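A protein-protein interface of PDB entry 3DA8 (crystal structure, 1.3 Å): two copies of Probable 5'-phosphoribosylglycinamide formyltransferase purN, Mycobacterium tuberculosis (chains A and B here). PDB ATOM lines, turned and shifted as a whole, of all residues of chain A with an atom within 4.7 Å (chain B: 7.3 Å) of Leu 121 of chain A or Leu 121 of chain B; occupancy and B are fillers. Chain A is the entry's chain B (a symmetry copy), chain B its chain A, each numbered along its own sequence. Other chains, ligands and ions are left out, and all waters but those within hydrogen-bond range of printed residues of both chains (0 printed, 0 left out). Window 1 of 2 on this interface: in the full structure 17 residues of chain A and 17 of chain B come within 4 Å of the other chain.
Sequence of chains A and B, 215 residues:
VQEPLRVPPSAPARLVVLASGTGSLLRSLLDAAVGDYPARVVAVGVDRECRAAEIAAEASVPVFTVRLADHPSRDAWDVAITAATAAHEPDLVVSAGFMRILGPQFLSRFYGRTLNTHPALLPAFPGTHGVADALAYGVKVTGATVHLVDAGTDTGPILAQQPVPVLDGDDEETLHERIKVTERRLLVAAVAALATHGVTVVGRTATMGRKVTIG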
ATOM      1  N   ALA A 120      -6.135  14.356  11.085  1.00  0.00           N
ATOM      2  CA  ALA A 120      -6.829  15.405  10.347  1.00  0.00           C
ATOM      3  C   ALA A 120      -8.282  14.990  10.294  1.00  0.00           C
ATOM      4  O   ALA A 120      -8.636  13.856  10.659  1.00  0.00           O
ATOM      5  CB  ALA A 120      -6.246  15.597   8.957  1.00  0.00           C
ATOM      6  N   LEU A 121      -9.135  15.920   9.868  1.00  0.00           N
ATOM      7  CA  LEU A 121     -10.540  15.613   9.585  1.00  0.00           C
ATOM      8  C   LEU A 121     -10.649  15.121   8.152  1.00  0.00           C
ATOM      9  O   LEU A 121     -10.848  15.898   7.208  1.00  0.00           O
ATOM     10  CB  LEU A 121     -11.433  16.845   9.802  1.00  0.00           C
ATOM     11  CG  LEU A 121     -11.494  17.379  11.231  1.00  0.00           C
ATOM     12  CD1 LEU A 121     -12.207  18.729  11.271  1.00  0.00           C
ATOM     13  CD2 LEU A 121     -12.189  16.399  12.170  1.00  0.00           C
ATOM     14  N   LEU A 122     -10.499  13.811   7.979  1.00  0.00           N
ATOM     15  CA  LEU A 122     -10.595  13.256   6.640  1.00  0.00           C
ATOM     16  C   LEU A 122     -11.959  13.645   6.051  1.00  0.00           C
ATOM     17  O   LEU A 122     -12.970  13.723   6.774  1.00  0.00           O
ATOM     18  CB  LEU A 122     -10.414  11.734   6.692  1.00  0.00           C
ATOM     19  CG  LEU A 122      -9.004  11.279   7.094  1.00  0.00           C
ATOM     20  CD1 LEU A 122      -8.970   9.772   7.255  1.00  0.00           C
ATOM     21  CD2 LEU A 122      -8.000  11.734   6.050  1.00  0.00           C
ATOM     22  N   PRO A 123     -12.018  13.870   4.731  1.00  0.00           N
ATOM     23  CA  PRO A 123     -10.982  13.578   3.722  1.00  0.00           C
ATOM     24  C   PRO A 123      -9.936  14.666   3.534  1.00  0.00           C
ATOM     25  O   PRO A 123      -9.087  14.520   2.661  1.00  0.00           O
ATOM     26  CB  PRO A 123     -11.795  13.395   2.437  1.00  0.00           C
ATOM     27  CG  PRO A 123     -12.975  14.275   2.628  1.00  0.00           C
ATOM     28  CD  PRO A 123     -13.307  14.237   4.109  1.00  0.00           C
ATOM     29  N   ALA A 124      -9.980  15.736   4.320  1.00  0.00           N
ATOM     30  CA  ALA A 124      -8.922  16.743   4.244  1.00  0.00           C
ATOM     31  C   ALA A 124      -7.610  16.162   4.768  1.00  0.00           C
ATOM     32  O   ALA A 124      -7.592  15.358   5.694  1.00  0.00           O
ATOM     33  CB  ALA A 124      -9.291  17.982   5.043  1.00  0.00           C
ATOM     34  N   VAL A 141      -9.215  25.163  11.841  1.00  0.00           N
ATOM     35  CA  VAL A 141      -9.760  23.995  12.511  1.00  0.00           C
ATOM     36  C   VAL A 141      -9.237  22.774  11.772  1.00  0.00           C
ATOM     37  O   VAL A 141      -9.392  22.680  10.558  1.00  0.00           O
ATOM     38  CB  VAL A 141     -11.305  23.984  12.478  1.00  0.00           C
ATOM     39  CG1 VAL A 141     -11.864  22.667  13.028  1.00  0.00           C
ATOM     40  CG2 VAL A 141     -11.884  25.163  13.248  1.00  0.00           C
ATOM     41  N   THR A 142      -8.625  21.855  12.519  1.00  0.00           N
ATOM     42  CA  THR A 142      -8.304  20.532  12.005  1.00  0.00           C
ATOM     43  C   THR A 142      -8.942  19.553  12.980  1.00  0.00           C
ATOM     44  O   THR A 142      -9.991  19.866  13.540  1.00  0.00           O
ATOM     45  CB  THR A 142      -6.776  20.381  11.802  1.00  0.00           C
ATOM     46  OG1 THR A 142      -6.515  19.109  11.219  1.00  0.00           O
ATOM     47  CG2 THR A 142      -5.959  20.587  13.090  1.00  0.00           C
ATOM     48  N   GLY A 143      -8.370  18.372  13.170  1.00  0.00           N
ATOM     49  CA  GLY A 143      -9.009  17.424  14.058  1.00  0.00           C
ATOM     50  C   GLY A 143      -8.418  16.054  13.952  1.00  0.00           C
ATOM     51  O   GLY A 143      -7.370  15.872  13.345  1.00  0.00           O
ATOM     52  N   ALA A 144      -9.122  15.099  14.546  1.00  0.00           N
ATOM     53  CA  ALA A 144      -8.747  13.692  14.487  1.00  0.00           C
ATOM     54  C   ALA A 144      -9.906  12.882  13.930  1.00  0.00           C
ATOM     55  O   ALA A 144     -11.073  13.209  14.144  1.00  0.00           O
ATOM     56  CB  ALA A 144      -8.377  13.180  15.869  1.00  0.00           C
ATOM     57  N   THR A 145      -9.554  11.791  13.260  1.00  0.00           N
ATOM     58  CA  THR A 145     -10.534  10.869  12.684  1.00  0.00           C
ATOM     59  C   THR A 145     -10.236   9.442  13.138  1.00  0.00           C
ATOM     60  O   THR A 145      -9.074   9.018  13.123  1.00  0.00           O
ATOM     61  CB  THR A 145     -10.459  10.906  11.141  1.00  0.00           C
ATOM     62  OG1 THR A 145     -10.774  12.228  10.696  1.00  0.00           O
ATOM     63  CG2 THR A 145     -11.443   9.940  10.473  1.00  0.00           C
ATOM     64  N   GLN A 161     -15.200  11.614  14.574  1.00  0.00           N
ATOM     65  CA  GLN A 161     -14.286  12.727  14.344  1.00  0.00           C
ATOM     66  C   GLN A 161     -14.453  13.749  15.450  1.00  0.00           C
ATOM     67  O   GLN A 161     -15.526  13.856  16.035  1.00  0.00           O
ATOM     68  CB  GLN A 161     -14.541  13.408  12.989  1.00  0.00           C
ATOM     69  CG  GLN A 161     -14.159  12.524  11.821  1.00  0.00           C
ATOM     70  CD  GLN A 161     -14.421  13.147  10.477  1.00  0.00           C
ATOM     71  OE1 GLN A 161     -15.543  13.544  10.183  1.00  0.00           O
ATOM     72  NE2 GLN A 161     -13.379  13.209   9.643  1.00  0.00           N
ATOM     73  N   GLN A 162     -13.403  14.520  15.716  1.00  0.00           N
ATOM     74  CA  GLN A 162     -13.482  15.588  16.692  1.00  0.00           C
ATOM     75  C   GLN A 162     -12.556  16.698  16.241  1.00  0.00           C
ATOM     76  O   GLN A 162     -11.415  16.437  15.883  1.00  0.00           O
ATOM     77  CB  GLN A 162     -13.047  15.076  18.068  1.00  0.00           C
ATOM     78  CG  GLN A 162     -13.225  16.098  19.197  1.00  0.00           C
ATOM     79  CD  GLN A 162     -14.683  16.270  19.661  1.00  0.00           C
ATOM     80  OE1 GLN A 162     -15.592  15.578  19.185  1.00  0.00           O
ATOM     81  NE2 GLN A 162     -14.903  17.185  20.604  1.00  0.00           N
ATOM     82  N   PRO A 163     -13.040  17.947  16.265  1.00  0.00           N
ATOM     83  CA  PRO A 163     -12.206  19.078  15.819  1.00  0.00           C
ATOM     84  C   PRO A 163     -11.157  19.491  16.843  1.00  0.00           C
ATOM     85  O   PRO A 163     -11.319  19.241  18.034  1.00  0.00           O
ATOM     86  CB  PRO A 163     -13.235  20.193  15.598  1.00  0.00           C
ATOM     87  CG  PRO A 163     -14.294  19.887  16.665  1.00  0.00           C
ATOM     88  CD  PRO A 163     -14.397  18.376  16.667  1.00  0.00           C
ATOM     89  N   HIS B 118     -18.305  29.794   3.350  1.00  0.00           N
ATOM     90  CA  HIS B 118     -18.553  28.502   2.722  1.00  0.00           C
ATOM     91  C   HIS B 118     -19.054  27.532   3.784  1.00  0.00           C
ATOM     92  O   HIS B 118     -18.483  27.501   4.881  1.00  0.00           O
ATOM     93  CB  HIS B 118     -17.259  27.996   2.091  1.00  0.00           C
ATOM     94  CG  HIS B 118     -17.442  26.755   1.292  1.00  0.00           C
ATOM     95  ND1 HIS B 118     -18.034  26.748   0.048  1.00  0.00           N
ATOM     96  CD2 HIS B 118     -17.131  25.469   1.571  1.00  0.00           C
ATOM     97  CE1 HIS B 118     -18.081  25.507  -0.409  1.00  0.00           C
ATOM     98  NE2 HIS B 118     -17.553  24.709   0.505  1.00  0.00           N
ATOM     99  N   PRO B 119     -20.073  26.709   3.454  1.00  0.00           N
ATOM    100  CA  PRO B 119     -20.636  25.791   4.440  1.00  0.00           C
ATOM    101  C   PRO B 119     -19.886  24.436   4.519  1.00  0.00           C
ATOM    102  O   PRO B 119     -20.520  23.378   4.539  1.00  0.00           O
ATOM    103  CB  PRO B 119     -22.071  25.613   3.947  1.00  0.00           C
ATOM    104  CG  PRO B 119     -21.949  25.687   2.476  1.00  0.00           C
ATOM    105  CD  PRO B 119     -20.882  26.719   2.215  1.00  0.00           C
ATOM    106  N   ALA B 120     -18.558  24.490   4.567  1.00  0.00           N
ATOM    107  CA  ALA B 120     -17.732  23.325   4.875  1.00  0.00           C
ATOM    108  C   ALA B 120     -16.452  23.863   5.470  1.00  0.00           C
ATOM    109  O   ALA B 120     -16.200  25.084   5.429  1.00  0.00           O
ATOM    110  CB  ALA B 120     -17.430  22.491   3.646  1.00  0.00           C
ATOM    111  N   LEU B 121     -15.627  22.967   6.026  1.00  0.00           N
ATOM    112  CA  LEU B 121     -14.286  23.331   6.486  1.00  0.00           C
ATOM    113  C   LEU B 121     -13.346  23.198   5.308  1.00  0.00           C
ATOM    114  O   LEU B 121     -12.776  22.141   5.052  1.00  0.00           O
ATOM    115  CB  LEU B 121     -13.834  22.428   7.644  1.00  0.00           C
ATOM    116  CG  LEU B 121     -14.653  22.569   8.933  1.00  0.00           C
ATOM    117  CD1 LEU B 121     -14.232  21.476   9.916  1.00  0.00           C
ATOM    118  CD2 LEU B 121     -14.486  23.952   9.551  1.00  0.00           C
ATOM    119  N   LEU B 122     -13.189  24.275   4.552  1.00  0.00           N
ATOM    120  CA  LEU B 122     -12.243  24.256   3.435  1.00  0.00           C
ATOM    121  C   LEU B 122     -10.863  23.830   3.952  1.00  0.00           C
ATOM    122  O   LEU B 122     -10.473  24.218   5.063  1.00  0.00           O
ATOM    123  CB  LEU B 122     -12.198  25.629   2.755  1.00  0.00           C
ATOM    124  CG  LEU B 122     -13.480  25.996   1.994  1.00  0.00           C
ATOM    125  CD1 LEU B 122     -13.438  27.440   1.525  1.00  0.00           C
ATOM    126  CD2 LEU B 122     -13.719  25.062   0.816  1.00  0.00           C
ATOM    127  N   PRO B 123     -10.107  23.062   3.157  1.00  0.00           N
ATOM    128  CA  PRO B 123     -10.313  22.732   1.745  1.00  0.00           C
ATOM    129  C   PRO B 123     -11.226  21.543   1.459  1.00  0.00           C
ATOM    130  O   PRO B 123     -11.360  21.171   0.296  1.00  0.00           O
ATOM    131  CB  PRO B 123      -8.898  22.410   1.257  1.00  0.00           C
ATOM    132  CG  PRO B 123      -8.241  21.818   2.469  1.00  0.00           C
ATOM    133  CD  PRO B 123      -8.774  22.632   3.628  1.00  0.00           C
ATOM    134  N   ALA B 124     -11.872  20.974   2.470  1.00  0.00           N
ATOM    135  CA  ALA B 124     -12.851  19.919   2.225  1.00  0.00           C
ATOM    136  C   ALA B 124     -14.115  20.470   1.566  1.00  0.00           C
ATOM    137  O   ALA B 124     -14.526  21.606   1.816  1.00  0.00           O
ATOM    138  CB  ALA B 124     -13.212  19.184   3.502  1.00  0.00           C
ATOM    139  N   PHE B 125     -14.736  19.628   0.742  1.00  0.00           N
ATOM    140  CA  PHE B 125     -16.066  19.854   0.152  1.00  0.00           C
ATOM    141  C   PHE B 125     -16.257  21.254  -0.435  1.00  0.00           C
ATOM    142  O   PHE B 125     -17.197  21.974  -0.077  1.00  0.00           O
ATOM    143  CB  PHE B 125     -17.156  19.483   1.167  1.00  0.00           C
ATOM    144  CG  PHE B 125     -16.953  18.109   1.735  1.00  0.00           C
ATOM    145  CD1 PHE B 125     -16.995  16.993   0.911  1.00  0.00           C
ATOM    146  CD2 PHE B 125     -16.653  17.933   3.078  1.00  0.00           C
ATOM    147  CE1 PHE B 125     -16.775  15.710   1.428  1.00  0.00           C
ATOM    148  CE2 PHE B 125     -16.427  16.648   3.608  1.00  0.00           C
ATOM    149  CZ  PHE B 125     -16.477  15.539   2.771  1.00  0.00           C
ATOM    150  N   PRO B 126     -15.386  21.632  -1.385  1.00  0.00           N
ATOM    151  CA  PRO B 126     -15.564  22.905  -2.076  1.00  0.00           C
ATOM    152  C   PRO B 126     -16.755  22.832  -3.045  1.00  0.00           C
ATOM    153  O   PRO B 126     -17.278  21.750  -3.331  1.00  0.00           O
ATOM    154  CB  PRO B 126     -14.261  23.047  -2.853  1.00  0.00           C
ATOM    155  CG  PRO B 126     -13.853  21.637  -3.149  1.00  0.00           C
ATOM    156  CD  PRO B 126     -14.244  20.861  -1.926  1.00  0.00           C
ATOM    157  N   VAL B 139     -18.753  12.012   6.728  1.00  0.00           N
ATOM    158  CA  VAL B 139     -17.989  12.665   7.790  1.00  0.00           C
ATOM    159  C   VAL B 139     -18.872  12.859   9.028  1.00  0.00           C
ATOM    160  O   VAL B 139     -20.112  12.897   8.937  1.00  0.00           O
ATOM    161  CB  VAL B 139     -17.381  14.021   7.352  1.00  0.00           C
ATOM    162  CG1 VAL B 139     -16.433  13.820   6.178  1.00  0.00           C
ATOM    163  CG2 VAL B 139     -18.458  15.084   7.028  1.00  0.00           C
ATOM    164  N   LYS B 140     -18.229  13.022  10.176  1.00  0.00           N
ATOM    165  CA  LYS B 140     -18.931  13.291  11.429  1.00  0.00           C
ATOM    166  C   LYS B 140     -18.783  14.732  11.886  1.00  0.00           C
ATOM    167  O   LYS B 140     -19.527  15.175  12.764  1.00  0.00           O
ATOM    168  CB  LYS B 140     -18.474  12.334  12.529  1.00  0.00           C
ATOM    169  CG  LYS B 140     -18.545  10.863  12.142  1.00  0.00           C
ATOM    170  CD  LYS B 140     -19.944  10.414  11.758  1.00  0.00           C
ATOM    171  CE  LYS B 140     -19.911   8.967  11.286  1.00  0.00           C
ATOM    172  NZ  LYS B 140     -21.174   8.608  10.595  1.00  0.00           N
ATOM    173  N   VAL B 141     -17.824  15.447  11.301  1.00  0.00           N
ATOM    174  CA  VAL B 141     -17.604  16.863  11.606  1.00  0.00           C
ATOM    175  C   VAL B 141     -17.464  17.589  10.288  1.00  0.00           C
ATOM    176  O   VAL B 141     -16.664  17.195   9.442  1.00  0.00           O
ATOM    177  CB  VAL B 141     -16.301  17.063  12.427  1.00  0.00           C
ATOM    178  CG1 VAL B 141     -15.970  18.548  12.561  1.00  0.00           C
ATOM    179  CG2 VAL B 141     -16.432  16.422  13.794  1.00  0.00           C
ATOM    180  N   THR B 142     -18.279  18.622  10.114  1.00  0.00           N
ATOM    181  CA  THR B 142     -18.104  19.561   9.018  1.00  0.00           C
ATOM    182  C   THR B 142     -17.999  20.943   9.659  1.00  0.00           C
ATOM    183  O   THR B 142     -17.501  21.031  10.779  1.00  0.00           O
ATOM    184  CB  THR B 142     -19.208  19.397   7.947  1.00  0.00           C
ATOM    185  OG1 THR B 142     -18.910  20.278   6.877  1.00  0.00           O
ATOM    186  CG2 THR B 142     -20.612  19.628   8.473  1.00  0.00           C
ATOM    187  N   GLY B 143     -18.430  22.011   8.995  1.00  0.00           N
ATOM    188  CA  GLY B 143     -18.297  23.327   9.604  1.00  0.00           C
ATOM    189  C   GLY B 143     -18.501  24.429   8.610  1.00  0.00           C
ATOM    190  O   GLY B 143     -19.022  24.192   7.518  1.00  0.00           O
ATOM    191  N   ALA B 144     -18.106  25.634   9.023  1.00  0.00           N
ATOM    192  CA  ALA B 144     -18.189  26.818   8.198  1.00  0.00           C
ATOM    193  C   ALA B 144     -16.833  27.491   8.124  1.00  0.00           C
ATOM    194  O   ALA B 144     -16.057  27.435   9.081  1.00  0.00           O
ATOM    195  CB  ALA B 144     -19.206  27.785   8.784  1.00  0.00           C
ATOM    196  N   THR B 145     -16.566  28.135   6.978  1.00  0.00           N
ATOM    197  CA  THR B 145     -15.341  28.873   6.760  1.00  0.00           C
ATOM    198  C   THR B 145     -15.652  30.294   6.320  1.00  0.00           C
ATOM    199  O   THR B 145     -16.528  30.503   5.480  1.00  0.00           O
ATOM    200  CB  THR B 145     -14.514  28.196   5.639  1.00  0.00           C
ATOM    201  OG1 THR B 145     -14.229  26.837   5.999  1.00  0.00           O
ATOM    202  CG2 THR B 145     -13.204  28.893   5.384  1.00  0.00           C
ATOM    203  N   ILE B 158      -7.786  31.699   4.652  1.00  0.00           N
ATOM    204  CA  ILE B 158      -8.827  31.425   5.620  1.00  0.00           C
ATOM    205  C   ILE B 158      -8.731  32.376   6.817  1.00  0.00           C
ATOM    206  O   ILE B 158      -7.674  32.504   7.434  1.00  0.00           O
ATOM    207  CB  ILE B 158      -8.758  29.961   6.056  1.00  0.00           C
ATOM    208  CG1 ILE B 158      -9.118  29.056   4.859  1.00  0.00           C
ATOM    209  CG2 ILE B 158      -9.677  29.718   7.255  1.00  0.00           C
ATOM    210  CD1 ILE B 158      -8.803  27.609   5.110  1.00  0.00           C
ATOM    211  N   ALA B 160     -11.385  32.461   9.408  1.00  0.00           N
ATOM    212  CA  ALA B 160     -12.004  31.876  10.595  1.00  0.00           C
ATOM    213  C   ALA B 160     -12.692  30.590  10.170  1.00  0.00           C
ATOM    214  O   ALA B 160     -13.200  30.497   9.050  1.00  0.00           O
ATOM    215  CB  ALA B 160     -13.021  32.840  11.188  1.00  0.00           C
ATOM    216  N   GLN B 161     -12.756  29.615  11.081  1.00  0.00           N
ATOM    217  CA  GLN B 161     -13.514  28.385  10.858  1.00  0.00           C
ATOM    218  C   GLN B 161     -14.149  27.963  12.144  1.00  0.00           C
ATOM    219  O   GLN B 161     -13.617  28.239  13.209  1.00  0.00           O
ATOM    220  CB  GLN B 161     -12.627  27.254  10.323  1.00  0.00           C
ATOM    221  CG  GLN B 161     -12.207  27.482   8.892  1.00  0.00           C
ATOM    222  CD  GLN B 161     -11.283  26.427   8.345  1.00  0.00           C
ATOM    223  OE1 GLN B 161     -10.247  26.120   8.946  1.00  0.00           O
ATOM    224  NE2 GLN B 161     -11.640  25.883   7.178  1.00  0.00           N
ATOM    225  N   GLN B 162     -15.273  27.266  12.045  1.00  0.00           N
ATOM    226  CA  GLN B 162     -15.911  26.680  13.224  1.00  0.00           C
ATOM    227  C   GLN B 162     -16.534  25.358  12.839  1.00  0.00           C
ATOM    228  O   GLN B 162     -17.226  25.283  11.839  1.00  0.00           O
ATOM    229  CB  GLN B 162     -16.986  27.624  13.774  1.00  0.00           C
ATOM    230  CG  GLN B 162     -17.656  27.158  15.077  1.00  0.00           C
ATOM    231  CD  GLN B 162     -16.749  27.317  16.286  1.00  0.00           C
ATOM    232  OE1 GLN B 162     -15.748  28.042  16.238  1.00  0.00           O
ATOM    233  NE2 GLN B 162     -17.095  26.643  17.373  1.00  0.00           N
ATOM    234  N   PRO B 163     -16.303  24.319  13.648  1.00  0.00           N
ATOM    235  CA  PRO B 163     -16.841  23.011  13.302  1.00  0.00           C
ATOM    236  C   PRO B 163     -18.319  22.897  13.644  1.00  0.00           C
ATOM    237  O   PRO B 163     -18.807  23.616  14.516  1.00  0.00           O
ATOM    238  CB  PRO B 163     -15.996  22.063  14.152  1.00  0.00           C
ATOM    239  CG  PRO B 163     -15.714  22.885  15.399  1.00  0.00           C
ATOM    240  CD  PRO B 163     -15.462  24.277  14.864  1.00  0.00           C
ATOM    241  N   VAL B 164     -18.997  21.965  12.973  1.00  0.00           N
ATOM    242  CA  VAL B 164     -20.420  21.682  13.128  1.00  0.00           C
ATOM    243  C   VAL B 164     -20.546  20.149  13.053  1.00  0.00           C
ATOM    244  O   VAL B 164     -20.006  19.550  12.131  1.00  0.00           O
ATOM    245  CB  VAL B 164     -21.250  22.346  11.981  1.00  0.00           C
ATOM    246  CG1 VAL B 164     -22.713  21.933  12.041  1.00  0.00           C
ATOM    247  CG2 VAL B 164     -21.145  23.872  12.045  1.00  0.00           C
ATOM    248  N   LEU B 186     -20.222  33.223  12.462  1.00  0.00           N
ATOM    249  CA  LEU B 186     -18.801  33.260  12.232  1.00  0.00           C
ATOM    250  C   LEU B 186     -18.435  34.485  11.394  1.00  0.00           C
ATOM    251  O   LEU B 186     -17.433  35.147  11.660  1.00  0.00           O
ATOM    252  CB  LEU B 186     -18.387  31.979  11.515  1.00  0.00           C
ATOM    253  CG  LEU B 186     -16.886  31.712  11.393  1.00  0.00           C
ATOM    254  CD1 LEU B 186     -16.274  31.473  12.777  1.00  0.00           C
ATOM    255  CD2 LEU B 186     -16.645  30.523  10.466  1.00  0.00           C
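N of Val 141 of chain B sits at hydrogen-bond distance from OE1 of Gln 161 of chain A, at 3.2 Å. OE1 of Gln 161 of chain A lies within hydrogen-bond range of N of Lys 140 of chain B (2.7 Å). The side-chain amide oxygen of Gln 161 of chain B sits at hydrogen-bond distance from the backbone NH of Val 141 of chain A (3.2 Å).
The backbone carbonyl oxygen of Leu 122 of chain A is in hydrogen-bond range of the side-chain amide nitrogen of Gln 161 of chain A. NE2 of His 118 of chain B is in hydrogen-bond range of O of Phe 125 of chain B (2.8 Å). The side-chain hydroxyl (OG1) of Thr 145 of chain A sits at hydrogen-bond distance from the side-chain amide nitrogen (NE2) of Gln 161 of chain A, 3.0 Å away. The side-chain hydroxyl of Thr 145 of chain A is in hydrogen-bond range of the backbone NH of Leu 122 of chain A, at 3.2 Å. O of Leu 122 of chain B lies within hydrogen-bond range of NE2 of Gln 161 of chain B, at 2.9 Å. NE2 of Gln 161 of chain B sits at hydrogen-bond distance from OG1 of Thr 145 of chain B, 3.0 Å away.
Among the printed residues, pairs that only touch across the chains: Gln 161 of chain A with Val 139 of chain B (3.4 Å), Leu 122 of chain A with Val 139 of chain B (3.5 Å), Pro 163 of chain A with Pro 163 of chain B (3.6 Å), Leu 121 of chain A with Leu 121 of chain B (3.7 Å), Pro 123 of chain A with Phe 125 of chain B (3.7 Å), Pro 123 of chain A with Val 139 of chain B (3.8 Å) and Leu 121 of chain A with Val 141 of chain B (3.98 Å).
Of the printed residues of chain B, Leu 121 of chain A touches Leu 121 and Val 141. Of the printed residues of chain B, Leu 122 of chain A touches Val 139 (3.5 Å). Printed residues of chain B within 4 Å of Val 141 of chain A: Gln 161. Thr 142 of chain A touches none of the printed residues of chain B. Of the printed residues of chain B, Gln 161 of chain A touches Val 139, Lys 140 and Val 141. Of the printed residues of chain B, Pro 163 of chain A touches Pro 163 (3.6 Å). Of chain A, only Leu 121 comes within 4 Å of Leu 121 of chain B. Of the printed residues of chain A, Lys 140 of chain B touches Gln 161 (2.7 Å). Ala 160 of chain B touches none of the printed residues of chain A. The nearest residue of chain A that does not touch Leu 121 of chain B is Val 141 of chain A (4.1 Å).
Of the 13 printed residues of chain A, 6 touch a printed residue of chain B. Hydrophobic or aromatic side chains of chain B that line the printed part of chain A: Leu 121, Phe 125, Val 139, Val 141 and Pro 163.
Leu 121 of chain B touches its own counterpart, Leu 121 of chain A. Leu 121 of chain A touches Val 141 of chain B, but with the chains exchanged Val 141 of chain A does not touch Leu 121 of chain B (4.1 Å). Val 141 of chain A touches Gln 161 of chain B, and with the chains exchanged Gln 161 of chain A touches Val 141 of chain B. Pro 163 of chain B touches its own counterpart, Pro 163 of chain A. Of the 10 pairs that touch across the chains among the printed residues, 4 have their exchanged pair printed and touching as well.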
